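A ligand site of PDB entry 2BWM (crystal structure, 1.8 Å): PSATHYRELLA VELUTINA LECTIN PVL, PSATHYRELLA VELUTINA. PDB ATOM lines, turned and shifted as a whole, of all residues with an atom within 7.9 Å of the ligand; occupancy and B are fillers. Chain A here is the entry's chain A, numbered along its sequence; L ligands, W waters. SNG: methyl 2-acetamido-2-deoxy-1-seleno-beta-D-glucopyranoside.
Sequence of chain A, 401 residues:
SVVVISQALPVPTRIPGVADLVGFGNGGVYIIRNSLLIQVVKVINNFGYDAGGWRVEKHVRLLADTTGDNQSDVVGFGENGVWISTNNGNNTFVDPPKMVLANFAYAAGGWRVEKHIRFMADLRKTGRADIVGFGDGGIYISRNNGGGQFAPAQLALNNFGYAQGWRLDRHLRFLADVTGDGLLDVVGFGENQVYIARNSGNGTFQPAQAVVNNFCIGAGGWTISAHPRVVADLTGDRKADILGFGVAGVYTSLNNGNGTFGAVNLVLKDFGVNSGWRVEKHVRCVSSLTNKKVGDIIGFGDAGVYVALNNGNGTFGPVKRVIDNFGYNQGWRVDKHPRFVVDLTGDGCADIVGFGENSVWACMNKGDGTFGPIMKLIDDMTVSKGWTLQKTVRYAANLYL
Water W1 lies within hydrogen-bond range of OD1 of Asn 80 (2.8 Å), O7 of the ligand (2.8 Å), NE1 of Trp 83 (2.9 Å) and N of Glu 79 (3.3 Å).
The backbone NH (N) of Trp 54 sits at hydrogen-bond distance from the backbone carbonyl oxygen (O) of Gly 48, 3.0 Å away.
OE1 of Glu 79 sits at hydrogen-bond distance from NE2 of His 59 (2.7 Å).
The side-chain carboxylate (OE2) of Glu 79 is in salt-bridge range of the side-chain amino group (NZ) of Lys 58 (2.8 Å).
ND1 of His 59 is in hydrogen-bond range of N of Arg 55.
CE1 of His 59 touches C8 of the ligand (3.6 Å).
Gly 78 touches the ligand (CA to O7, 3.5 Å).
Asn 80 touches the ligand (OD1 to SE, 3.7 Å).
Hydrophobic or aromatic side chains within 4 Å of the ligand: Trp 54 and His 59.
Within 4 Å of the ligand: Asn 46, Gly 52, Trp 54, His 59, Gly 78, Glu 79 and Asn 80.
The nearest printed residue that does not touch the ligand is Gly 53 (4.02 Å).
The side-chain amide oxygen (OD1) of Asn 46 lies within hydrogen-bond range of an oxygen (O3) of the ligand, 2.6 Å away.
The backbone carbonyl oxygen of Gly 52 is in hydrogen-bond range of a nitrogen (N2) of the ligand (2.8 Å).
The indole nitrogen (NE1) of Trp 54 sits at hydrogen-bond distance from an oxygen (O3) of the ligand, 2.8 Å away.
N of Glu 79 is in hydrogen-bond range of O7 of the ligand (2.8 Å).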
ATOM      1  N   ASN A  45      27.790 -31.240  22.479  1.00  0.00           N
ATOM      2  CA  ASN A  45      27.107 -32.089  23.475  1.00  0.00           C
ATOM      3  C   ASN A  45      25.756 -31.504  23.815  1.00  0.00           C
ATOM      4  O   ASN A  45      25.440 -31.206  24.973  1.00  0.00           O
ATOM      5  CB  ASN A  45      27.998 -32.266  24.706  1.00  0.00           C
ATOM      6  CG  ASN A  45      27.442 -33.280  25.660  1.00  0.00           C
ATOM      7  OD1 ASN A  45      27.514 -33.079  26.880  1.00  0.00           O
ATOM      8  ND2 ASN A  45      26.936 -34.388  25.142  1.00  0.00           N
ATOM      9  N   ASN A  46      24.941 -31.366  22.787  1.00  0.00           N
ATOM     10  CA  ASN A  46      23.645 -30.752  22.901  1.00  0.00           C
ATOM     11  C   ASN A  46      22.875 -31.049  21.606  1.00  0.00           C
ATOM     12  O   ASN A  46      23.431 -31.709  20.691  1.00  0.00           O
ATOM     13  CB  ASN A  46      23.810 -29.244  23.187  1.00  0.00           C
ATOM     14  CG  ASN A  46      22.766 -28.707  24.140  1.00  0.00           C
ATOM     15  OD1 ASN A  46      21.595 -28.929  23.943  1.00  0.00           O
ATOM     16  ND2 ASN A  46      23.204 -28.030  25.230  1.00  0.00           N
ATOM     17  N   PHE A  47      21.628 -30.553  21.547  1.00  0.00           N
ATOM     18  CA  PHE A  47      20.700 -30.777  20.416  1.00  0.00           C
ATOM     19  C   PHE A  47      20.432 -32.258  20.162  1.00  0.00           C
ATOM     20  O   PHE A  47      20.145 -32.654  19.041  1.00  0.00           O
ATOM     21  CB  PHE A  47      21.264 -30.112  19.135  1.00  0.00           C
ATOM     22  CG  PHE A  47      21.537 -28.636  19.244  1.00  0.00           C
ATOM     23  CD1 PHE A  47      20.496 -27.743  19.128  1.00  0.00           C
ATOM     24  CD2 PHE A  47      22.838 -28.126  19.349  1.00  0.00           C
ATOM     25  CE1 PHE A  47      20.741 -26.374  19.151  1.00  0.00           C
ATOM     26  CE2 PHE A  47      23.080 -26.800  19.423  1.00  0.00           C
ATOM     27  CZ  PHE A  47      22.045 -25.904  19.263  1.00  0.00           C
ATOM     28  N   GLY A  48      20.523 -33.085  21.222  1.00  0.00           N
ATOM     29  CA  GLY A  48      20.306 -34.527  21.095  1.00  0.00           C
ATOM     30  C   GLY A  48      19.151 -35.030  21.969  1.00  0.00           C
ATOM     31  O   GLY A  48      18.740 -34.400  22.952  1.00  0.00           O
ATOM     32  N   ALA A  51      20.923 -35.492  24.964  1.00  0.00           N
ATOM     33  CA  ALA A  51      21.804 -34.363  25.215  1.00  0.00           C
ATOM     34  C   ALA A  51      20.955 -33.116  25.024  1.00  0.00           C
ATOM     35  O   ALA A  51      20.979 -32.447  23.990  1.00  0.00           O
ATOM     36  CB  ALA A  51      23.018 -34.379  24.288  1.00  0.00           C
ATOM     37  N   GLY A  52      20.133 -32.848  26.043  1.00  0.00           N
ATOM     38  CA  GLY A  52      19.231 -31.700  26.042  1.00  0.00           C
ATOM     39  C   GLY A  52      17.772 -31.988  25.882  1.00  0.00           C
ATOM     40  O   GLY A  52      16.964 -31.074  25.855  1.00  0.00           O
ATOM     41  N   GLY A  53      17.407 -33.269  25.758  1.00  0.00           N
ATOM     42  CA  GLY A  53      16.024 -33.645  25.694  1.00  0.00           C
ATOM     43  C   GLY A  53      15.299 -33.234  24.423  1.00  0.00           C
ATOM     44  O   GLY A  53      14.113 -32.890  24.428  1.00  0.00           O
ATOM     45  N   TRP A  54      16.031 -33.264  23.302  1.00  0.00           N
ATOM     46  CA  TRP A  54      15.474 -32.824  22.016  1.00  0.00           C
ATOM     47  C   TRP A  54      14.608 -33.921  21.439  1.00  0.00           C
ATOM     48  O   TRP A  54      14.953 -35.126  21.504  1.00  0.00           O
ATOM     49  CB  TRP A  54      16.594 -32.400  21.056  1.00  0.00           C
ATOM     50  CG  TRP A  54      17.226 -31.097  21.499  1.00  0.00           C
ATOM     51  CD1 TRP A  54      18.031 -30.910  22.602  1.00  0.00           C
ATOM     52  CD2 TRP A  54      17.002 -29.810  20.945  1.00  0.00           C
ATOM     53  NE1 TRP A  54      18.321 -29.585  22.732  1.00  0.00           N
ATOM     54  CE2 TRP A  54      17.696 -28.881  21.741  1.00  0.00           C
ATOM     55  CE3 TRP A  54      16.302 -29.335  19.812  1.00  0.00           C
ATOM     56  CZ2 TRP A  54      17.735 -27.510  21.441  1.00  0.00           C
ATOM     57  CZ3 TRP A  54      16.310 -27.972  19.539  1.00  0.00           C
ATOM     58  CH2 TRP A  54      17.022 -27.071  20.354  1.00  0.00           C
ATOM     59  N   ARG A  55      13.485 -33.516  20.850  1.00  0.00           N
ATOM     60  CA  ARG A  55      12.449 -34.419  20.401  1.00  0.00           C
ATOM     61  C   ARG A  55      11.960 -34.033  19.017  1.00  0.00           C
ATOM     62  O   ARG A  55      11.595 -32.859  18.799  1.00  0.00           O
ATOM     63  CB  ARG A  55      11.258 -34.398  21.382  1.00  0.00           C
ATOM     64  CG  ARG A  55      11.589 -34.892  22.774  1.00  0.00           C
ATOM     65  CD  ARG A  55      11.847 -36.383  22.765  1.00  0.00           C
ATOM     66  NE  ARG A  55      12.079 -36.888  24.124  1.00  0.00           N
ATOM     67  CZ  ARG A  55      13.271 -36.949  24.725  1.00  0.00           C
ATOM     68  NH1 ARG A  55      14.358 -36.551  24.116  1.00  0.00           N
ATOM     69  NH2 ARG A  55      13.379 -37.479  25.935  1.00  0.00           N
ATOM     70  N   LYS A  58       8.611 -32.223  18.983  1.00  0.00           N
ATOM     71  CA  LYS A  58       8.439 -30.934  19.612  1.00  0.00           C
ATOM     72  C   LYS A  58       9.378 -29.834  19.127  1.00  0.00           C
ATOM     73  O   LYS A  58       9.115 -28.680  19.365  1.00  0.00           O
ATOM     74  CB  LYS A  58       8.636 -31.051  21.116  1.00  0.00           C
ATOM     75  CG  LYS A  58       7.658 -31.970  21.814  1.00  0.00           C
ATOM     76  CD  LYS A  58       7.889 -31.967  23.339  1.00  0.00           C
ATOM     77  CE  LYS A  58       7.467 -30.706  24.013  1.00  0.00           C
ATOM     78  NZ  LYS A  58       7.798 -30.710  25.506  1.00  0.00           N
ATOM     79  N   HIS A  59      10.506 -30.218  18.552  1.00  0.00           N
ATOM     80  CA  HIS A  59      11.633 -29.307  18.294  1.00  0.00           C
ATOM     81  C   HIS A  59      12.136 -29.474  16.871  1.00  0.00           C
ATOM     82  O   HIS A  59      11.957 -30.535  16.265  1.00  0.00           O
ATOM     83  CB  HIS A  59      12.786 -29.623  19.286  1.00  0.00           C
ATOM     84  CG  HIS A  59      12.349 -29.699  20.723  1.00  0.00           C
ATOM     85  ND1 HIS A  59      12.548 -30.823  21.508  1.00  0.00           N
ATOM     86  CD2 HIS A  59      11.623 -28.848  21.471  1.00  0.00           C
ATOM     87  CE1 HIS A  59      12.018 -30.616  22.713  1.00  0.00           C
ATOM     88  NE2 HIS A  59      11.446 -29.423  22.725  1.00  0.00           N
ATOM     89  N   ARG A  61      15.523 -28.897  14.213  1.00  0.00           N
ATOM     90  CA  ARG A  61      17.012 -28.761  14.183  1.00  0.00           C
ATOM     91  C   ARG A  61      17.447 -28.624  12.731  1.00  0.00           C
ATOM     92  O   ARG A  61      17.158 -29.520  11.898  1.00  0.00           O
ATOM     93  CB  ARG A  61      17.652 -29.986  14.834  1.00  0.00           C
ATOM     94  CG  ARG A  61      17.594 -29.875  16.401  1.00  0.00           C
ATOM     95  CD  ARG A  61      17.824 -31.154  17.083  1.00  0.00           C
ATOM     96  NE  ARG A  61      16.739 -32.096  16.960  1.00  0.00           N
ATOM     97  CZ  ARG A  61      16.746 -33.368  17.394  1.00  0.00           C
ATOM     98  NH1 ARG A  61      17.786 -33.856  18.071  1.00  0.00           N
ATOM     99  NH2 ARG A  61      15.686 -34.119  17.213  1.00  0.00           N
ATOM    100  N   GLY A  76      18.723 -24.645  16.596  1.00  0.00           N
ATOM    101  CA  GLY A  76      17.650 -25.469  17.137  1.00  0.00           C
ATOM    102  C   GLY A  76      16.511 -24.688  17.716  1.00  0.00           C
ATOM    103  O   GLY A  76      16.729 -23.766  18.519  1.00  0.00           O
ATOM    104  N   PHE A  77      15.276 -25.021  17.309  1.00  0.00           N
ATOM    105  CA  PHE A  77      14.074 -24.449  17.881  1.00  0.00           C
ATOM    106  C   PHE A  77      13.713 -25.412  19.001  1.00  0.00           C
ATOM    107  O   PHE A  77      13.146 -26.459  18.758  1.00  0.00           O
ATOM    108  CB  PHE A  77      12.953 -24.319  16.829  1.00  0.00           C
ATOM    109  CG  PHE A  77      13.324 -23.433  15.629  1.00  0.00           C
ATOM    110  CD1 PHE A  77      12.821 -22.140  15.534  1.00  0.00           C
ATOM    111  CD2 PHE A  77      14.134 -23.909  14.601  1.00  0.00           C
ATOM    112  CE1 PHE A  77      13.154 -21.318  14.443  1.00  0.00           C
ATOM    113  CE2 PHE A  77      14.440 -23.082  13.493  1.00  0.00           C
ATOM    114  CZ  PHE A  77      13.936 -21.790  13.434  1.00  0.00           C
ATOM    115  N   GLY A  78      14.125 -25.062  20.222  1.00  0.00           N
ATOM    116  CA  GLY A  78      13.947 -25.892  21.380  1.00  0.00           C
ATOM    117  C   GLY A  78      12.668 -25.701  22.136  1.00  0.00           C
ATOM    118  O   GLY A  78      11.631 -25.319  21.590  1.00  0.00           O
ATOM    119  N   GLU A  79      12.727 -25.978  23.444  1.00  0.00           N
ATOM    120  CA  GLU A  79      11.520 -25.895  24.218  1.00  0.00           C
ATOM    121  C   GLU A  79      11.059 -24.446  24.437  1.00  0.00           C
ATOM    122  O   GLU A  79       9.860 -24.186  24.417  1.00  0.00           O
ATOM    123  CB  GLU A  79      11.713 -26.552  25.573  1.00  0.00           C
ATOM    124  CG  GLU A  79      10.410 -26.767  26.325  1.00  0.00           C
ATOM    125  CD  GLU A  79       9.551 -27.884  25.798  1.00  0.00           C
ATOM    126  OE1 GLU A  79       9.907 -28.546  24.796  1.00  0.00           O
ATOM    127  OE2 GLU A  79       8.478 -28.146  26.417  1.00  0.00           O
ATOM    128  N   ASN A  80      12.017 -23.547  24.734  1.00  0.00           N
ATOM    129  CA  ASN A  80      11.658 -22.161  25.108  1.00  0.00           C
ATOM    130  C   ASN A  80      12.280 -21.064  24.298  1.00  0.00           C
ATOM    131  O   ASN A  80      12.152 -19.882  24.670  1.00  0.00           O
ATOM    132  CB  ASN A  80      12.098 -21.790  26.547  1.00  0.00           C
ATOM    133  CG  ASN A  80      12.359 -22.942  27.394  1.00  0.00           C
ATOM    134  OD1 ASN A  80      13.515 -23.319  27.596  1.00  0.00           O
ATOM    135  ND2 ASN A  80      11.288 -23.530  27.931  1.00  0.00           N
ATOM    136  N   GLY A  81      12.979 -21.399  23.209  1.00  0.00           N
ATOM    137  CA  GLY A  81      13.562 -20.403  22.380  1.00  0.00           C
ATOM    138  C   GLY A  81      14.379 -20.988  21.252  1.00  0.00           C
ATOM    139  O   GLY A  81      14.472 -22.256  21.110  1.00  0.00           O
ATOM    140  N   VAL A  82      15.052 -20.076  20.529  1.00  0.00           N
ATOM    141  CA  VAL A  82      15.962 -20.485  19.411  1.00  0.00           C
ATOM    142  C   VAL A  82      17.405 -20.477  19.937  1.00  0.00           C
ATOM    143  O   VAL A  82      17.846 -19.455  20.432  1.00  0.00           O
ATOM    144  CB  VAL A  82      15.780 -19.633  18.159  1.00  0.00           C
ATOM    145  CG1 VAL A  82      16.663 -20.161  17.026  1.00  0.00           C
ATOM    146  CG2 VAL A  82      14.290 -19.635  17.749  1.00  0.00           C
ATOM    147  N   TRP A  83      18.094 -21.607  19.759  1.00  0.00           N
ATOM    148  CA  TRP A  83      19.453 -21.821  20.188  1.00  0.00           C
ATOM    149  C   TRP A  83      20.389 -21.935  18.982  1.00  0.00           C
ATOM    150  O   TRP A  83      20.037 -22.585  17.991  1.00  0.00           O
ATOM    151  CB  TRP A  83      19.566 -23.118  20.971  1.00  0.00           C
ATOM    152  CG  TRP A  83      18.828 -23.156  22.259  1.00  0.00           C
ATOM    153  CD1 TRP A  83      17.536 -23.498  22.458  1.00  0.00           C
ATOM    154  CD2 TRP A  83      19.373 -22.880  23.544  1.00  0.00           C
ATOM    155  NE1 TRP A  83      17.212 -23.412  23.793  1.00  0.00           N
ATOM    156  CE2 TRP A  83      18.342 -23.069  24.485  1.00  0.00           C
ATOM    157  CE3 TRP A  83      20.637 -22.479  23.996  1.00  0.00           C
ATOM    158  CZ2 TRP A  83      18.535 -22.844  25.841  1.00  0.00           C
ATOM    159  CZ3 TRP A  83      20.827 -22.286  25.331  1.00  0.00           C
ATOM    160  CH2 TRP A  83      19.786 -22.455  26.244  1.00  0.00           C
ATOM    161  N   ASP A  95      30.107 -24.570  21.968  1.00  0.00           N
ATOM    162  CA  ASP A  95      29.358 -25.503  22.819  1.00  0.00           C
ATOM    163  C   ASP A  95      29.566 -24.999  24.247  1.00  0.00           C
ATOM    164  O   ASP A  95      30.704 -25.018  24.720  1.00  0.00           O
ATOM    165  CB  ASP A  95      29.897 -26.945  22.629  1.00  0.00           C
ATOM    166  CG  ASP A  95      29.067 -28.036  23.361  1.00  0.00           C
ATOM    167  OD1 ASP A  95      27.973 -27.745  23.882  1.00  0.00           O
ATOM    168  OD2 ASP A  95      29.544 -29.231  23.394  1.00  0.00           O
ATOM    169  N   PRO A  96      28.494 -24.585  24.927  1.00  0.00           N
ATOM    170  CA  PRO A  96      27.080 -24.682  24.526  1.00  0.00           C
ATOM    171  C   PRO A  96      26.627 -23.652  23.514  1.00  0.00           C
ATOM    172  O   PRO A  96      27.227 -22.577  23.370  1.00  0.00           O
ATOM    173  CB  PRO A  96      26.331 -24.478  25.863  1.00  0.00           C
ATOM    174  CG  PRO A  96      27.230 -23.543  26.616  1.00  0.00           C
ATOM    175  CD  PRO A  96      28.610 -24.061  26.321  1.00  0.00           C
ATOM    176  N   PRO A  97      25.460 -23.913  22.886  1.00  0.00           N
ATOM    177  CA  PRO A  97      24.806 -22.904  22.125  1.00  0.00           C
ATOM    178  C   PRO A  97      24.265 -21.799  23.045  1.00  0.00           C
ATOM    179  O   PRO A  97      24.145 -21.991  24.247  1.00  0.00           O
ATOM    180  CB  PRO A  97      23.612 -23.653  21.487  1.00  0.00           C
ATOM    181  CG  PRO A  97      23.309 -24.733  22.491  1.00  0.00           C
ATOM    182  CD  PRO A  97      24.684 -25.150  22.992  1.00  0.00           C
ATOM    183  N   MET A  99      20.984 -18.907  23.435  1.00  0.00           N
ATOM    184  CA  MET A  99      19.608 -18.647  23.052  1.00  0.00           C
ATOM    185  C   MET A  99      19.492 -17.233  22.484  1.00  0.00           C
ATOM    186  O   MET A  99      19.767 -16.254  23.189  1.00  0.00           O
ATOM    187  CB  MET A  99      18.635 -18.818  24.218  1.00  0.00           C
ATOM    188  CG  MET A  99      17.162 -18.782  23.704  1.00  0.00           C
ATOM    189  SD  MET A  99      15.924 -18.586  24.978  1.00  0.00           S
ATOM    190  CE  MET A  99      15.888 -20.287  25.390  1.00  0.00           C
ATOM    191  N   ALA A 105       9.001 -21.423  19.500  1.00  0.00           N
ATOM    192  CA  ALA A 105       9.275 -22.643  20.296  1.00  0.00           C
ATOM    193  C   ALA A 105       8.010 -23.175  20.931  1.00  0.00           C
ATOM    194  O   ALA A 105       7.003 -22.464  21.049  1.00  0.00           O
ATOM    195  CB  ALA A 105      10.326 -22.370  21.397  1.00  0.00           C
HETATM  196  C1  SNG L   1      16.994 -27.225  27.681  1.00  0.00           C
HETATM  197  C2  SNG L   1      17.361 -27.350  26.210  1.00  0.00           C
HETATM  198  C3  SNG L   1      18.820 -27.867  26.188  1.00  0.00           C
HETATM  199  C4  SNG L   1      19.735 -26.928  26.952  1.00  0.00           C
HETATM  200  C5  SNG L   1      19.212 -26.622  28.326  1.00  0.00           C
HETATM  201  C6  SNG L   1      20.010 -25.481  28.950  1.00  0.00           C
HETATM  202  C7  SNG L   1      15.548 -27.981  24.674  1.00  0.00           C
HETATM  203  C8  SNG L   1      14.900 -28.974  24.007  1.00  0.00           C
HETATM  204  CM  SNG L   1      15.129 -26.579  29.857  1.00  0.00           C
HETATM  205  N2  SNG L   1      16.550 -28.337  25.471  1.00  0.00           N
HETATM  206  O3  SNG L   1      19.298 -28.011  24.862  1.00  0.00           O
HETATM  207  O4  SNG L   1      21.060 -27.481  27.126  1.00  0.00           O
HETATM  208  O5  SNG L   1      17.812 -26.243  28.290  1.00  0.00           O
HETATM  209  O6  SNG L   1      19.449 -25.160  30.252  1.00  0.00           O
HETATM  210  O7  SNG L   1      15.183 -26.830  24.550  1.00  0.00           O
HETATM  211 SE   SNG L   1      15.166 -26.602  27.875  1.00  0.00          SE
HETATM  212  O   HOH W   1      14.758 -24.113  25.253  1.00  0.00           O
HETATM  213  O   HOH W   2      21.280 -29.958  28.036  1.00  0.00           O
HETATM  214  O   HOH W   3      18.073 -30.000  29.448  1.00  0.00           O
